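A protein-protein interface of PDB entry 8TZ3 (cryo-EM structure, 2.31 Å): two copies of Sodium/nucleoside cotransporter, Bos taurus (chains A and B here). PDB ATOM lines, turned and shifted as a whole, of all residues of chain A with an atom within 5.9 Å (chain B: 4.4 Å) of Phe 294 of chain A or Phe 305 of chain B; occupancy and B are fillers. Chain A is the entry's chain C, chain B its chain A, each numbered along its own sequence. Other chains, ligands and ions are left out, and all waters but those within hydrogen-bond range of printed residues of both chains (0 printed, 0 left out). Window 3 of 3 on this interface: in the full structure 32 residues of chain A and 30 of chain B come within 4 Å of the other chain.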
ATOM      1  N   ASP A 289     -20.309  26.506   8.680  1.00  0.00           N
ATOM      2  CA  ASP A 289     -19.838  26.011   7.394  1.00  0.00           C
ATOM      3  C   ASP A 289     -18.347  25.702   7.402  1.00  0.00           C
ATOM      4  O   ASP A 289     -17.895  24.832   6.653  1.00  0.00           O
ATOM      5  CB  ASP A 289     -20.153  27.028   6.303  1.00  0.00           C
ATOM      6  CG  ASP A 289     -21.621  27.071   5.943  1.00  0.00           C
ATOM      7  OD1 ASP A 289     -22.378  26.178   6.374  1.00  0.00           O
ATOM      8  OD2 ASP A 289     -22.022  28.008   5.227  1.00  0.00           O
ATOM      9  N   ALA A 290     -17.567  26.416   8.212  1.00  0.00           N
ATOM     10  CA  ALA A 290     -16.150  26.108   8.339  1.00  0.00           C
ATOM     11  C   ALA A 290     -15.932  24.707   8.899  1.00  0.00           C
ATOM     12  O   ALA A 290     -15.013  23.999   8.478  1.00  0.00           O
ATOM     13  CB  ALA A 290     -15.474  27.150   9.219  1.00  0.00           C
ATOM     14  N   GLY A 291     -16.761  24.296   9.856  1.00  0.00           N
ATOM     15  CA  GLY A 291     -16.668  22.943  10.369  1.00  0.00           C
ATOM     16  C   GLY A 291     -17.240  21.909   9.421  1.00  0.00           C
ATOM     17  O   GLY A 291     -16.714  20.800   9.307  1.00  0.00           O
ATOM     18  N   ALA A 292     -18.327  22.254   8.735  1.00  0.00           N
ATOM     19  CA  ALA A 292     -18.964  21.329   7.806  1.00  0.00           C
ATOM     20  C   ALA A 292     -18.130  21.123   6.549  1.00  0.00           C
ATOM     21  O   ALA A 292     -18.198  20.062   5.922  1.00  0.00           O
ATOM     22  CB  ALA A 292     -20.353  21.845   7.450  1.00  0.00           C
ATOM     23  N   SER A 293     -17.345  22.124   6.156  1.00  0.00           N
ATOM     24  CA  SER A 293     -16.576  22.012   4.925  1.00  0.00           C
ATOM     25  C   SER A 293     -15.300  21.203   5.108  1.00  0.00           C
ATOM     26  O   SER A 293     -14.660  20.843   4.116  1.00  0.00           O
ATOM     27  CB  SER A 293     -16.243  23.398   4.384  1.00  0.00           C
ATOM     28  OG  SER A 293     -15.544  23.299   3.162  1.00  0.00           O
ATOM     29  N   PHE A 294     -14.900  20.913   6.345  1.00  0.00           N
ATOM     30  CA  PHE A 294     -13.767  20.019   6.532  1.00  0.00           C
ATOM     31  C   PHE A 294     -14.213  18.580   6.749  1.00  0.00           C
ATOM     32  O   PHE A 294     -13.644  17.654   6.165  1.00  0.00           O
ATOM     33  CB  PHE A 294     -12.890  20.467   7.699  1.00  0.00           C
ATOM     34  CG  PHE A 294     -11.846  19.455   8.051  1.00  0.00           C
ATOM     35  CD1 PHE A 294     -10.771  19.245   7.207  1.00  0.00           C
ATOM     36  CD2 PHE A 294     -11.968  18.664   9.176  1.00  0.00           C
ATOM     37  CE1 PHE A 294      -9.836  18.302   7.492  1.00  0.00           C
ATOM     38  CE2 PHE A 294     -11.028  17.718   9.465  1.00  0.00           C
ATOM     39  CZ  PHE A 294      -9.957  17.533   8.624  1.00  0.00           C
ATOM     40  N   VAL A 295     -15.220  18.373   7.597  1.00  0.00           N
ATOM     41  CA  VAL A 295     -15.671  17.021   7.900  1.00  0.00           C
ATOM     42  C   VAL A 295     -16.317  16.382   6.678  1.00  0.00           C
ATOM     43  O   VAL A 295     -16.129  15.190   6.416  1.00  0.00           O
ATOM     44  CB  VAL A 295     -16.616  17.049   9.118  1.00  0.00           C
ATOM     45  CG1 VAL A 295     -17.232  15.695   9.388  1.00  0.00           C
ATOM     46  CG2 VAL A 295     -15.859  17.523  10.331  1.00  0.00           C
ATOM     47  N   PHE A 296     -17.062  17.162   5.899  1.00  0.00           N
ATOM     48  CA  PHE A 296     -17.782  16.646   4.743  1.00  0.00           C
ATOM     49  C   PHE A 296     -17.251  17.162   3.414  1.00  0.00           C
ATOM     50  O   PHE A 296     -17.727  16.725   2.364  1.00  0.00           O
ATOM     51  CB  PHE A 296     -19.268  16.971   4.867  1.00  0.00           C
ATOM     52  CG  PHE A 296     -19.897  16.416   6.090  1.00  0.00           C
ATOM     53  CD1 PHE A 296     -19.905  15.066   6.315  1.00  0.00           C
ATOM     54  CD2 PHE A 296     -20.479  17.239   7.020  1.00  0.00           C
ATOM     55  CE1 PHE A 296     -20.469  14.552   7.426  1.00  0.00           C
ATOM     56  CE2 PHE A 296     -21.049  16.725   8.138  1.00  0.00           C
ATOM     57  CZ  PHE A 296     -21.045  15.379   8.345  1.00  0.00           C
ATOM     58  N   GLY A 297     -16.287  18.064   3.429  1.00  0.00           N
ATOM     59  CA  GLY A 297     -15.654  18.512   2.215  1.00  0.00           C
ATOM     60  C   GLY A 297     -16.343  19.683   1.556  1.00  0.00           C
ATOM     61  O   GLY A 297     -17.388  20.172   1.980  1.00  0.00           O
ATOM     62  N   HIS B 303     -16.163  12.980  -0.041  1.00  0.00           N
ATOM     63  CA  HIS B 303     -16.184  13.430   1.350  1.00  0.00           C
ATOM     64  C   HIS B 303     -15.039  12.720   2.070  1.00  0.00           C
ATOM     65  O   HIS B 303     -15.230  11.729   2.774  1.00  0.00           O
ATOM     66  CB  HIS B 303     -17.551  13.169   1.984  1.00  0.00           C
ATOM     67  CG  HIS B 303     -18.695  13.512   1.085  1.00  0.00           C
ATOM     68  ND1 HIS B 303     -19.116  14.805   0.872  1.00  0.00           N
ATOM     69  CD2 HIS B 303     -19.487  12.731   0.319  1.00  0.00           C
ATOM     70  CE1 HIS B 303     -20.122  14.804   0.023  1.00  0.00           C
ATOM     71  NE2 HIS B 303     -20.370  13.557  -0.328  1.00  0.00           N
ATOM     72  N   PHE B 304     -13.838  13.271   1.890  1.00  0.00           N
ATOM     73  CA  PHE B 304     -12.604  12.590   2.265  1.00  0.00           C
ATOM     74  C   PHE B 304     -12.551  12.269   3.755  1.00  0.00           C
ATOM     75  O   PHE B 304     -12.346  11.114   4.141  1.00  0.00           O
ATOM     76  CB  PHE B 304     -11.414  13.456   1.849  1.00  0.00           C
ATOM     77  CG  PHE B 304     -10.084  12.902   2.240  1.00  0.00           C
ATOM     78  CD1 PHE B 304      -9.499  11.899   1.502  1.00  0.00           C
ATOM     79  CD2 PHE B 304      -9.408  13.396   3.337  1.00  0.00           C
ATOM     80  CE1 PHE B 304      -8.281  11.390   1.855  1.00  0.00           C
ATOM     81  CE2 PHE B 304      -8.186  12.889   3.693  1.00  0.00           C
ATOM     82  CZ  PHE B 304      -7.622  11.886   2.952  1.00  0.00           C
ATOM     83  N   PHE B 305     -12.711  13.274   4.612  1.00  0.00           N
ATOM     84  CA  PHE B 305     -12.531  13.031   6.037  1.00  0.00           C
ATOM     85  C   PHE B 305     -13.601  12.098   6.589  1.00  0.00           C
ATOM     86  O   PHE B 305     -13.296  11.192   7.371  1.00  0.00           O
ATOM     87  CB  PHE B 305     -12.517  14.352   6.807  1.00  0.00           C
ATOM     88  CG  PHE B 305     -12.316  14.188   8.277  1.00  0.00           C
ATOM     89  CD1 PHE B 305     -11.057  14.001   8.796  1.00  0.00           C
ATOM     90  CD2 PHE B 305     -13.385  14.208   9.142  1.00  0.00           C
ATOM     91  CE1 PHE B 305     -10.874  13.840  10.133  1.00  0.00           C
ATOM     92  CE2 PHE B 305     -13.201  14.045  10.479  1.00  0.00           C
ATOM     93  CZ  PHE B 305     -11.944  13.862  10.976  1.00  0.00           C
ATOM     94  N   ALA B 306     -14.856  12.294   6.196  1.00  0.00           N
ATOM     95  CA  ALA B 306     -15.934  11.522   6.794  1.00  0.00           C
ATOM     96  C   ALA B 306     -15.990  10.103   6.243  1.00  0.00           C
ATOM     97  O   ALA B 306     -16.241   9.155   6.993  1.00  0.00           O
ATOM     98  CB  ALA B 306     -17.266  12.235   6.582  1.00  0.00           C
ATOM     99  N   PHE B 307     -15.754   9.933   4.944  1.00  0.00           N
ATOM    100  CA  PHE B 307     -15.978   8.657   4.280  1.00  0.00           C
ATOM    101  C   PHE B 307     -14.697   7.919   3.929  1.00  0.00           C
ATOM    102  O   PHE B 307     -14.772   6.826   3.365  1.00  0.00           O
ATOM    103  CB  PHE B 307     -16.824   8.858   3.014  1.00  0.00           C
ATOM    104  CG  PHE B 307     -18.250   9.237   3.281  1.00  0.00           C
ATOM    105  CD1 PHE B 307     -18.728   9.313   4.565  1.00  0.00           C
ATOM    106  CD2 PHE B 307     -19.118   9.508   2.246  1.00  0.00           C
ATOM    107  CE1 PHE B 307     -20.007   9.654   4.816  1.00  0.00           C
ATOM    108  CE2 PHE B 307     -20.415   9.846   2.505  1.00  0.00           C
ATOM    109  CZ  PHE B 307     -20.856   9.920   3.791  1.00  0.00           C
ATOM    110  N   LYS B 308     -13.541   8.464   4.253  1.00  0.00           N
ATOM    111  CA  LYS B 308     -12.276   7.772   4.043  1.00  0.00           C
ATOM    112  C   LYS B 308     -11.393   7.726   5.283  1.00  0.00           C
ATOM    113  O   LYS B 308     -10.720   6.720   5.505  1.00  0.00           O
ATOM    114  CB  LYS B 308     -11.517   8.419   2.885  1.00  0.00           C
ATOM    115  CG  LYS B 308     -10.155   7.855   2.666  1.00  0.00           C
ATOM    116  CD  LYS B 308      -9.743   7.968   1.248  1.00  0.00           C
ATOM    117  CE  LYS B 308      -8.322   7.512   1.075  1.00  0.00           C
ATOM    118  NZ  LYS B 308      -8.116   6.890  -0.234  1.00  0.00           N
ATOM    119  N   VAL B 309     -11.392   8.771   6.102  1.00  0.00           N
ATOM    120  CA  VAL B 309     -10.503   8.838   7.260  1.00  0.00           C
ATOM    121  C   VAL B 309     -11.124   8.180   8.479  1.00  0.00           C
ATOM    122  O   VAL B 309     -10.442   7.489   9.236  1.00  0.00           O
ATOM    123  CB  VAL B 309     -10.113  10.305   7.549  1.00  0.00           C
ATOM    124  CG1 VAL B 309      -9.303  10.418   8.824  1.00  0.00           C
ATOM    125  CG2 VAL B 309      -9.352  10.880   6.402  1.00  0.00           C
ATOM    126  N   LEU B 310     -12.417   8.384   8.704  1.00  0.00           N
ATOM    127  CA  LEU B 310     -13.047   7.777   9.870  1.00  0.00           C
ATOM    128  C   LEU B 310     -13.220   6.273   9.720  1.00  0.00           C
ATOM    129  O   LEU B 310     -13.268   5.581  10.751  1.00  0.00           O
ATOM    130  CB  LEU B 310     -14.378   8.479  10.166  1.00  0.00           C
ATOM    131  CG  LEU B 310     -14.304   9.945  10.615  1.00  0.00           C
ATOM    132  CD1 LEU B 310     -15.680  10.553  10.745  1.00  0.00           C
ATOM    133  CD2 LEU B 310     -13.542  10.136  11.907  1.00  0.00           C
ATOM    134  N   PHE B 403      -3.278  12.586   6.956  1.00  0.00           N
ATOM    135  CA  PHE B 403      -3.088  14.014   6.743  1.00  0.00           C
ATOM    136  C   PHE B 403      -1.778  14.297   6.018  1.00  0.00           C
ATOM    137  O   PHE B 403      -1.715  15.183   5.161  1.00  0.00           O
ATOM    138  CB  PHE B 403      -3.119  14.749   8.080  1.00  0.00           C
ATOM    139  CG  PHE B 403      -4.459  14.767   8.749  1.00  0.00           C
ATOM    140  CD1 PHE B 403      -5.604  14.377   8.085  1.00  0.00           C
ATOM    141  CD2 PHE B 403      -4.571  15.199  10.050  1.00  0.00           C
ATOM    142  CE1 PHE B 403      -6.819  14.410   8.711  1.00  0.00           C
ATOM    143  CE2 PHE B 403      -5.780  15.235  10.678  1.00  0.00           C
ATOM    144  CZ  PHE B 403      -6.908  14.842  10.012  1.00  0.00           C
ATOM    145  N   ILE B 471     -15.397  12.603  17.435  1.00  0.00           N
ATOM    146  CA  ILE B 471     -14.362  13.259  16.641  1.00  0.00           C
ATOM    147  C   ILE B 471     -14.992  14.238  15.657  1.00  0.00           C
ATOM    148  O   ILE B 471     -14.560  15.388  15.537  1.00  0.00           O
ATOM    149  CB  ILE B 471     -13.483  12.215  15.921  1.00  0.00           C
ATOM    150  CG1 ILE B 471     -12.639  11.418  16.913  1.00  0.00           C
ATOM    151  CG2 ILE B 471     -12.567  12.867  14.913  1.00  0.00           C
ATOM    152  CD1 ILE B 471     -12.066  10.134  16.354  1.00  0.00           C
ATOM    153  N   LEU B 475     -15.044  18.612  15.903  1.00  0.00           N
ATOM    154  CA  LEU B 475     -14.362  19.365  14.857  1.00  0.00           C
ATOM    155  C   LEU B 475     -15.300  20.346  14.164  1.00  0.00           C
ATOM    156  O   LEU B 475     -14.879  21.438  13.775  1.00  0.00           O
ATOM    157  CB  LEU B 475     -13.743  18.402  13.848  1.00  0.00           C
ATOM    158  CG  LEU B 475     -12.383  17.787  14.160  1.00  0.00           C
ATOM    159  CD1 LEU B 475     -12.160  16.632  13.226  1.00  0.00           C
ATOM    160  CD2 LEU B 475     -11.269  18.788  14.032  1.00  0.00           C
ATOM    161  N   LEU B 479     -14.171  24.275  14.847  1.00  0.00           N
ATOM    162  CA  LEU B 479     -13.801  25.048  13.670  1.00  0.00           C
ATOM    163  C   LEU B 479     -14.822  26.132  13.358  1.00  0.00           C
ATOM    164  O   LEU B 479     -14.493  27.110  12.684  1.00  0.00           O
ATOM    165  CB  LEU B 479     -13.615  24.115  12.479  1.00  0.00           C
ATOM    166  CG  LEU B 479     -12.412  23.169  12.525  1.00  0.00           C
ATOM    167  CD1 LEU B 479     -12.473  22.211  11.377  1.00  0.00           C
ATOM    168  CD2 LEU B 479     -11.106  23.914  12.504  1.00  0.00           C
ATOM    169  N   GLN B 545      -3.958  18.851  11.401  1.00  0.00           N
ATOM    170  CA  GLN B 545      -4.479  19.258  10.101  1.00  0.00           C
ATOM    171  C   GLN B 545      -3.778  20.512   9.589  1.00  0.00           C
ATOM    172  O   GLN B 545      -3.549  20.656   8.384  1.00  0.00           O
ATOM    173  CB  GLN B 545      -5.993  19.462  10.201  1.00  0.00           C
ATOM    174  CG  GLN B 545      -6.637  20.294   9.104  1.00  0.00           C
ATOM    175  CD  GLN B 545      -6.450  19.691   7.739  1.00  0.00           C
ATOM    176  OE1 GLN B 545      -6.307  18.476   7.593  1.00  0.00           O
ATOM    177  NE2 GLN B 545      -6.444  20.536   6.725  1.00  0.00           N
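ND1 of His 303 of chain B lies within hydrogen-bond range of O of Phe 296 of chain A (2.8 Å). O of Val 295 of chain A lies close to N of Ala 306 of chain B.
N of Leu 310 of chain B is in hydrogen-bond range of O of Phe 305 of chain B (3.2 Å).
Among the printed residues, merely in contact across the chains: Phe 294 of chain A with Gln 545 of chain B (3.5 Å), Phe 294 of chain A with Phe 305 of chain B (3.5 Å), Ala 290 of chain A with Leu 479 of chain B (3.6 Å), Val 295 of chain A with Phe 305 of chain B (3.7 Å), Phe 296 of chain A with Ala 306 of chain B (3.9 Å) and Gly 291 of chain A with Leu 479 of chain B (3.9 Å).
Of the printed residues of chain B, Phe 294 of chain A touches Phe 305 (3.5 Å) and Gln 545 (3.5 Å). Of the printed residues of chain B, Val 295 of chain A touches Phe 305 and Ala 306. Of the printed residues of chain A, His 303 of chain B touches Phe 296. Of the printed residues of chain A, Gln 545 of chain B touches Phe 294 (3.5 Å). Printed residues of chain B within 4 Å of Ala 290 of chain A: Leu 479 (3.6 Å). Asp 289 of chain A touches none of the printed residues of chain B. Gly 297 of chain A touches none of the printed residues of chain B. The nearest printed residue of chain B that does not touch Phe 294 of chain A is Leu 475 of chain B (4.1 Å). The nearest residue of chain A that does not touch Phe 305 of chain B is Phe 296 of chain A (5.4 Å).
Hydrophobic or aromatic side chains of chain A that line the printed part of chain B: Ala 290, Phe 294 and Phe 296. Hydrophobic or aromatic side chains of chain B within 4 Å of the printed part of chain A: His 303, Phe 305, Ala 306 and Leu 479. Among the printed residues, no Asp or Glu carboxylate lies within 4 Å of a Lys or Arg side-chain nitrogen of the other chain.
No position is printed for both chains. Of the 8 pairs that touch across the chains among the printed residues, none has its exchanged pair printed and touching as well.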
